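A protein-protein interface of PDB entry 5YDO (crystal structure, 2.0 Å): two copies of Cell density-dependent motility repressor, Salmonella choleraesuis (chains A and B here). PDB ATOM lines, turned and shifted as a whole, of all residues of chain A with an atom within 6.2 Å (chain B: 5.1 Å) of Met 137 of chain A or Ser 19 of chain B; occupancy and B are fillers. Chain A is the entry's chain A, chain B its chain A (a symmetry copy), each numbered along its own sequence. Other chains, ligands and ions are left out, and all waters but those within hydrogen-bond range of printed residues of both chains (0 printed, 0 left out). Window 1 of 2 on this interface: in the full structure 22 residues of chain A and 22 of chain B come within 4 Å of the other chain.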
ATOM      1  N   HIS A  16     -26.959  -3.961  20.810  1.00  0.00           N
ATOM      2  CA  HIS A  16     -26.432  -5.310  20.607  1.00  0.00           C
ATOM      3  C   HIS A  16     -24.967  -5.278  20.196  1.00  0.00           C
ATOM      4  O   HIS A  16     -24.151  -6.049  20.715  1.00  0.00           O
ATOM      5  CB  HIS A  16     -27.253  -6.044  19.548  1.00  0.00           C
ATOM      6  CG  HIS A  16     -28.636  -6.402  19.992  1.00  0.00           C
ATOM      7  ND1 HIS A  16     -28.886  -7.326  20.984  1.00  0.00           N
ATOM      8  CD2 HIS A  16     -29.848  -5.968  19.570  1.00  0.00           C
ATOM      9  CE1 HIS A  16     -30.191  -7.440  21.160  1.00  0.00           C
ATOM     10  NE2 HIS A  16     -30.797  -6.627  20.314  1.00  0.00           N
ATOM     11  N   SER A  17     -24.617  -4.392  19.268  1.00  0.00           N
ATOM     12  CA  SER A  17     -23.271  -4.323  18.719  1.00  0.00           C
ATOM     13  C   SER A  17     -22.267  -3.686  19.670  1.00  0.00           C
ATOM     14  O   SER A  17     -21.096  -3.547  19.303  1.00  0.00           O
ATOM     15  CB  SER A  17     -23.296  -3.550  17.397  1.00  0.00           C
ATOM     16  OG  SER A  17     -24.264  -2.510  17.444  1.00  0.00           O
ATOM     17  N   TYR A 107     -24.922  -6.494   9.564  1.00  0.00           N
ATOM     18  CA  TYR A 107     -25.815  -6.270  10.687  1.00  0.00           C
ATOM     19  C   TYR A 107     -27.258  -6.194  10.191  1.00  0.00           C
ATOM     20  O   TYR A 107     -27.525  -6.069   8.994  1.00  0.00           O
ATOM     21  CB  TYR A 107     -25.447  -4.980  11.419  1.00  0.00           C
ATOM     22  CG  TYR A 107     -24.084  -4.982  12.072  1.00  0.00           C
ATOM     23  CD1 TYR A 107     -22.936  -4.718  11.336  1.00  0.00           C
ATOM     24  CD2 TYR A 107     -23.949  -5.229  13.430  1.00  0.00           C
ATOM     25  CE1 TYR A 107     -21.683  -4.709  11.938  1.00  0.00           C
ATOM     26  CE2 TYR A 107     -22.708  -5.221  14.041  1.00  0.00           C
ATOM     27  CZ  TYR A 107     -21.579  -4.959  13.288  1.00  0.00           C
ATOM     28  OH  TYR A 107     -20.344  -4.949  13.898  1.00  0.00           O
ATOM     29  N   SER A 135     -27.002 -10.651  11.230  1.00  0.00           N
ATOM     30  CA  SER A 135     -27.191 -10.783  12.667  1.00  0.00           C
ATOM     31  C   SER A 135     -26.914  -9.442  13.328  1.00  0.00           C
ATOM     32  O   SER A 135     -26.153  -8.621  12.806  1.00  0.00           O
ATOM     33  CB  SER A 135     -26.279 -11.857  13.266  1.00  0.00           C
ATOM     34  OG  SER A 135     -26.281 -11.783  14.683  1.00  0.00           O
ATOM     35  N   SER A 136     -27.529  -9.238  14.493  1.00  0.00           N
ATOM     36  CA  SER A 136     -27.292  -8.027  15.266  1.00  0.00           C
ATOM     37  C   SER A 136     -26.025  -8.105  16.111  1.00  0.00           C
ATOM     38  O   SER A 136     -25.446  -7.062  16.439  1.00  0.00           O
ATOM     39  CB  SER A 136     -28.498  -7.743  16.166  1.00  0.00           C
ATOM     40  OG  SER A 136     -28.664  -6.353  16.379  1.00  0.00           O
ATOM     41  N   MET A 137     -25.574  -9.309  16.457  1.00  0.00           N
ATOM     42  CA  MET A 137     -24.446  -9.479  17.367  1.00  0.00           C
ATOM     43  C   MET A 137     -23.132  -9.242  16.634  1.00  0.00           C
ATOM     44  O   MET A 137     -22.841  -9.914  15.638  1.00  0.00           O
ATOM     45  CB  MET A 137     -24.470 -10.877  17.978  1.00  0.00           C
ATOM     46  CG  MET A 137     -23.642 -11.021  19.244  1.00  0.00           C
ATOM     47  SD  MET A 137     -23.750 -12.695  19.908  1.00  0.00           S
ATOM     48  CE  MET A 137     -25.507 -13.008  19.738  1.00  0.00           C
ATOM     49  N   SER A 138     -22.335  -8.294  17.133  1.00  0.00           N
ATOM     50  CA  SER A 138     -21.021  -8.038  16.549  1.00  0.00           C
ATOM     51  C   SER A 138     -20.136  -9.278  16.605  1.00  0.00           C
ATOM     52  O   SER A 138     -19.416  -9.579  15.647  1.00  0.00           O
ATOM     53  CB  SER A 138     -20.341  -6.875  17.272  1.00  0.00           C
ATOM     54  OG  SER A 138     -20.843  -5.622  16.839  1.00  0.00           O
ATOM     55  N   GLU A 139     -20.179 -10.011  17.720  1.00  0.00           N
ATOM     56  CA  GLU A 139     -19.258 -11.128  17.902  1.00  0.00           C
ATOM     57  C   GLU A 139     -19.658 -12.330  17.062  1.00  0.00           C
ATOM     58  O   GLU A 139     -18.808 -13.165  16.742  1.00  0.00           O
ATOM     59  CB  GLU A 139     -19.183 -11.518  19.376  1.00  0.00           C
ATOM     60  CG  GLU A 139     -18.704 -10.400  20.278  1.00  0.00           C
ATOM     61  CD  GLU A 139     -19.796  -9.389  20.583  1.00  0.00           C
ATOM     62  OE1 GLU A 139     -20.974  -9.797  20.681  1.00  0.00           O
ATOM     63  OE2 GLU A 139     -19.476  -8.188  20.711  1.00  0.00           O
ATOM     64  N   LEU A 140     -20.939 -12.444  16.713  1.00  0.00           N
ATOM     65  CA  LEU A 140     -21.358 -13.490  15.792  1.00  0.00           C
ATOM     66  C   LEU A 140     -20.864 -13.197  14.380  1.00  0.00           C
ATOM     67  O   LEU A 140     -20.310 -14.076  13.709  1.00  0.00           O
ATOM     68  CB  LEU A 140     -22.883 -13.630  15.828  1.00  0.00           C
ATOM     69  CG  LEU A 140     -23.511 -14.809  15.087  1.00  0.00           C
ATOM     70  CD1 LEU A 140     -22.666 -16.053  15.254  1.00  0.00           C
ATOM     71  CD2 LEU A 140     -24.930 -15.058  15.585  1.00  0.00           C
ATOM     72  N   LEU A 141     -21.040 -11.957  13.915  1.00  0.00           N
ATOM     73  CA  LEU A 141     -20.506 -11.573  12.612  1.00  0.00           C
ATOM     74  C   LEU A 141     -18.996 -11.769  12.559  1.00  0.00           C
ATOM     75  O   LEU A 141     -18.452 -12.220  11.545  1.00  0.00           O
ATOM     76  CB  LEU A 141     -20.846 -10.115  12.315  1.00  0.00           C
ATOM     77  CG  LEU A 141     -22.314  -9.780  12.044  1.00  0.00           C
ATOM     78  CD1 LEU A 141     -22.432  -8.291  11.796  1.00  0.00           C
ATOM     79  CD2 LEU A 141     -22.846 -10.573  10.861  1.00  0.00           C
ATOM     80  N   LYS A 142     -18.304 -11.402  13.639  1.00  0.00           N
ATOM     81  CA  LYS A 142     -16.850 -11.553  13.700  1.00  0.00           C
ATOM     82  C   LYS A 142     -16.425 -13.008  13.547  1.00  0.00           C
ATOM     83  O   LYS A 142     -15.495 -13.314  12.787  1.00  0.00           O
ATOM     84  CB  LYS A 142     -16.331 -10.959  15.013  1.00  0.00           C
ATOM     85  CG  LYS A 142     -14.850 -11.136  15.276  1.00  0.00           C
ATOM     86  CD  LYS A 142     -14.590 -10.955  16.770  1.00  0.00           C
ATOM     87  CE  LYS A 142     -13.125 -11.019  17.110  1.00  0.00           C
ATOM     88  NZ  LYS A 142     -12.879 -10.686  18.539  1.00  0.00           N
ATOM     89  N   ALA B  14     -32.653 -17.471  17.847  1.00  0.00           N
ATOM     90  CA  ALA B  14     -31.840 -18.237  18.777  1.00  0.00           C
ATOM     91  C   ALA B  14     -31.808 -17.537  20.126  1.00  0.00           C
ATOM     92  O   ALA B  14     -31.747 -16.306  20.193  1.00  0.00           O
ATOM     93  CB  ALA B  14     -30.412 -18.416  18.242  1.00  0.00           C
ATOM     94  N   ALA B  15     -31.853 -18.326  21.197  1.00  0.00           N
ATOM     95  CA  ALA B  15     -31.766 -17.763  22.538  1.00  0.00           C
ATOM     96  C   ALA B  15     -30.461 -16.994  22.706  1.00  0.00           C
ATOM     97  O   ALA B  15     -29.462 -17.270  22.037  1.00  0.00           O
ATOM     98  CB  ALA B  15     -31.874 -18.867  23.588  1.00  0.00           C
ATOM     99  N   HIS B  16     -30.487 -16.001  23.599  1.00  0.00           N
ATOM    100  CA  HIS B  16     -29.318 -15.148  23.808  1.00  0.00           C
ATOM    101  C   HIS B  16     -28.103 -15.962  24.228  1.00  0.00           C
ATOM    102  O   HIS B  16     -26.997 -15.753  23.716  1.00  0.00           O
ATOM    103  CB  HIS B  16     -29.620 -14.084  24.863  1.00  0.00           C
ATOM    104  CG  HIS B  16     -30.591 -13.039  24.411  1.00  0.00           C
ATOM    105  ND1 HIS B  16     -30.298 -12.128  23.419  1.00  0.00           N
ATOM    106  CD2 HIS B  16     -31.848 -12.751  24.824  1.00  0.00           C
ATOM    107  CE1 HIS B  16     -31.334 -11.330  23.235  1.00  0.00           C
ATOM    108  NE2 HIS B  16     -32.288 -11.686  24.076  1.00  0.00           N
ATOM    109  N   SER B  17     -28.291 -16.895  25.158  1.00  0.00           N
ATOM    110  CA  SER B  17     -27.197 -17.678  25.714  1.00  0.00           C
ATOM    111  C   SER B  17     -26.688 -18.756  24.768  1.00  0.00           C
ATOM    112  O   SER B  17     -25.779 -19.504  25.142  1.00  0.00           O
ATOM    113  CB  SER B  17     -27.643 -18.313  27.035  1.00  0.00           C
ATOM    114  OG  SER B  17     -29.018 -18.669  26.979  1.00  0.00           O
ATOM    115  N   LEU B  18     -27.233 -18.846  23.555  1.00  0.00           N
ATOM    116  CA  LEU B  18     -26.917 -19.933  22.635  1.00  0.00           C
ATOM    117  C   LEU B  18     -26.433 -19.476  21.264  1.00  0.00           C
ATOM    118  O   LEU B  18     -25.841 -20.289  20.543  1.00  0.00           O
ATOM    119  CB  LEU B  18     -28.151 -20.835  22.459  1.00  0.00           C
ATOM    120  CG  LEU B  18     -28.133 -22.051  21.533  1.00  0.00           C
ATOM    121  CD1 LEU B  18     -26.962 -22.957  21.879  1.00  0.00           C
ATOM    122  CD2 LEU B  18     -29.442 -22.809  21.635  1.00  0.00           C
ATOM    123  N   SER B  19     -26.643 -18.212  20.884  1.00  0.00           N
ATOM    124  CA  SER B  19     -26.396 -17.793  19.505  1.00  0.00           C
ATOM    125  C   SER B  19     -24.930 -17.948  19.118  1.00  0.00           C
ATOM    126  O   SER B  19     -24.607 -18.601  18.120  1.00  0.00           O
ATOM    127  CB  SER B  19     -26.845 -16.346  19.309  1.00  0.00           C
ATOM    128  OG  SER B  19     -28.216 -16.189  19.626  1.00  0.00           O
ATOM    129  N   LEU B  20     -24.023 -17.347  19.894  1.00  0.00           N
ATOM    130  CA  LEU B  20     -22.624 -17.316  19.476  1.00  0.00           C
ATOM    131  C   LEU B  20     -21.998 -18.706  19.482  1.00  0.00           C
ATOM    132  O   LEU B  20     -21.190 -19.030  18.605  1.00  0.00           O
ATOM    133  CB  LEU B  20     -21.824 -16.364  20.365  1.00  0.00           C
ATOM    134  CG  LEU B  20     -20.358 -16.184  19.955  1.00  0.00           C
ATOM    135  CD1 LEU B  20     -20.233 -15.896  18.466  1.00  0.00           C
ATOM    136  CD2 LEU B  20     -19.703 -15.075  20.753  1.00  0.00           C
ATOM    137  N   GLY B  21     -22.355 -19.547  20.453  1.00  0.00           N
ATOM    138  CA  GLY B  21     -21.727 -20.855  20.536  1.00  0.00           C
ATOM    139  C   GLY B  21     -22.126 -21.802  19.421  1.00  0.00           C
ATOM    140  O   GLY B  21     -21.324 -22.639  18.998  1.00  0.00           O
ATOM    141  N   LEU B  22     -23.354 -21.681  18.920  1.00  0.00           N
ATOM    142  CA  LEU B  22     -23.938 -22.666  18.018  1.00  0.00           C
ATOM    143  C   LEU B  22     -23.999 -22.227  16.561  1.00  0.00           C
ATOM    144  O   LEU B  22     -23.752 -23.042  15.669  1.00  0.00           O
ATOM    145  CB  LEU B  22     -25.350 -23.021  18.494  1.00  0.00           C
ATOM    146  CG  LEU B  22     -26.184 -23.939  17.612  1.00  0.00           C
ATOM    147  CD1 LEU B  22     -25.573 -25.329  17.580  1.00  0.00           C
ATOM    148  CD2 LEU B  22     -27.608 -23.980  18.123  1.00  0.00           C
ATOM    149  N   LEU B  23     -24.318 -20.959  16.290  1.00  0.00           N
ATOM    150  CA  LEU B  23     -24.554 -20.536  14.909  1.00  0.00           C
ATOM    151  C   LEU B  23     -23.327 -20.668  14.015  1.00  0.00           C
ATOM    152  O   LEU B  23     -23.474 -21.164  12.884  1.00  0.00           O
ATOM    153  CB  LEU B  23     -25.106 -19.104  14.884  1.00  0.00           C
ATOM    154  CG  LEU B  23     -26.632 -18.985  14.851  1.00  0.00           C
ATOM    155  CD1 LEU B  23     -27.158 -19.488  13.511  1.00  0.00           C
ATOM    156  CD2 LEU B  23     -27.300 -19.718  16.009  1.00  0.00           C
ATOM    157  N   PRO B  24     -22.118 -20.254  14.418  1.00  0.00           N
ATOM    158  CA  PRO B  24     -20.966 -20.427  13.513  1.00  0.00           C
ATOM    159  C   PRO B  24     -20.714 -21.869  13.111  1.00  0.00           C
ATOM    160  O   PRO B  24     -20.333 -22.125  11.964  1.00  0.00           O
ATOM    161  CB  PRO B  24     -19.795 -19.855  14.327  1.00  0.00           C
ATOM    162  CG  PRO B  24     -20.424 -18.887  15.251  1.00  0.00           C
ATOM    163  CD  PRO B  24     -21.746 -19.492  15.623  1.00  0.00           C
ATOM    164  N   ALA B  40     -31.501 -12.660  17.967  1.00  0.00           N
ATOM    165  CA  ALA B  40     -31.445 -13.154  19.334  1.00  0.00           C
ATOM    166  C   ALA B  40     -32.756 -12.847  20.041  1.00  0.00           C
ATOM    167  O   ALA B  40     -33.284 -11.735  19.930  1.00  0.00           O
ATOM    168  CB  ALA B  40     -30.274 -12.519  20.084  1.00  0.00           C
ATOM    169  N   GLU B 139     -21.536 -14.548  26.743  1.00  0.00           N
ATOM    170  CA  GLU B 139     -20.157 -14.103  26.568  1.00  0.00           C
ATOM    171  C   GLU B 139     -19.852 -12.874  27.407  1.00  0.00           C
ATOM    172  O   GLU B 139     -18.688 -12.626  27.736  1.00  0.00           O
ATOM    173  CB  GLU B 139     -19.874 -13.818  25.095  1.00  0.00           C
ATOM    174  CG  GLU B 139     -20.067 -15.020  24.194  1.00  0.00           C
ATOM    175  CD  GLU B 139     -21.530 -15.284  23.881  1.00  0.00           C
ATOM    176  OE1 GLU B 139     -22.302 -14.306  23.777  1.00  0.00           O
ATOM    177  OE2 GLU B 139     -21.906 -16.468  23.753  1.00  0.00           O
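The side-chain hydroxyl (OG) of Ser 135 of chain A is in hydrogen-bond range of the backbone NH (N) of Met 137 of chain A (3.1 Å). The side-chain hydroxyl (OG) of Ser 19 of chain B is in hydrogen-bond range of the backbone carbonyl oxygen (O) of Ala 15 of chain B.
Met 137 of chain A touches Ser 19 of chain B (CE to CB, 3.6 Å). O of Glu 139 of chain A touches CD1 of Leu 20 of chain B, 3.5 Å away. Leu 20 of chain B touches Leu 140 of chain A. Leu 23 of chain B touches Leu 140 of chain A (CB to CD1, 3.9 Å). Leu 140 of chain A touches Pro 24 of chain B.
Met 137 of chain A touches one residue of chain B. Ser 19 of chain B touches one residue of chain A. Of the printed residues of chain A, Leu 20 of chain B touches Glu 139 and Leu 140. Of the printed residues of chain A, Pro 24 of chain B touches Leu 140. Printed residues of chain B within 4 Å of Glu 139 of chain A: Leu 20 (3.5 Å). Of the printed residues of chain A, Leu 23 of chain B touches Leu 140 (3.9 Å). The nearest residue of chain A that does not touch Ser 19 of chain B is Leu 140 of chain A (4.3 Å). The nearest printed residue of chain A that does not touch Pro 24 of chain B is Glu 139 of chain A (6.1 Å).
Of the 11 printed residues of chain A, 3 touch a printed residue of chain B. Of the 13 printed residues of chain B, 4 touch a printed residue of chain A. Printed residues of chain B that touch a printed residue of chain A: Ser 19, Leu 20, Leu 23 and Pro 24. Along chain B the printed residues that touch a printed residue of chain A span positions 19 to 24. Among the printed residues, no Asp or Glu carboxylate lies within 4 Å of a Lys or Arg side-chain nitrogen of the other chain.
Positions printed for both chains: 16, 17 and 139.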
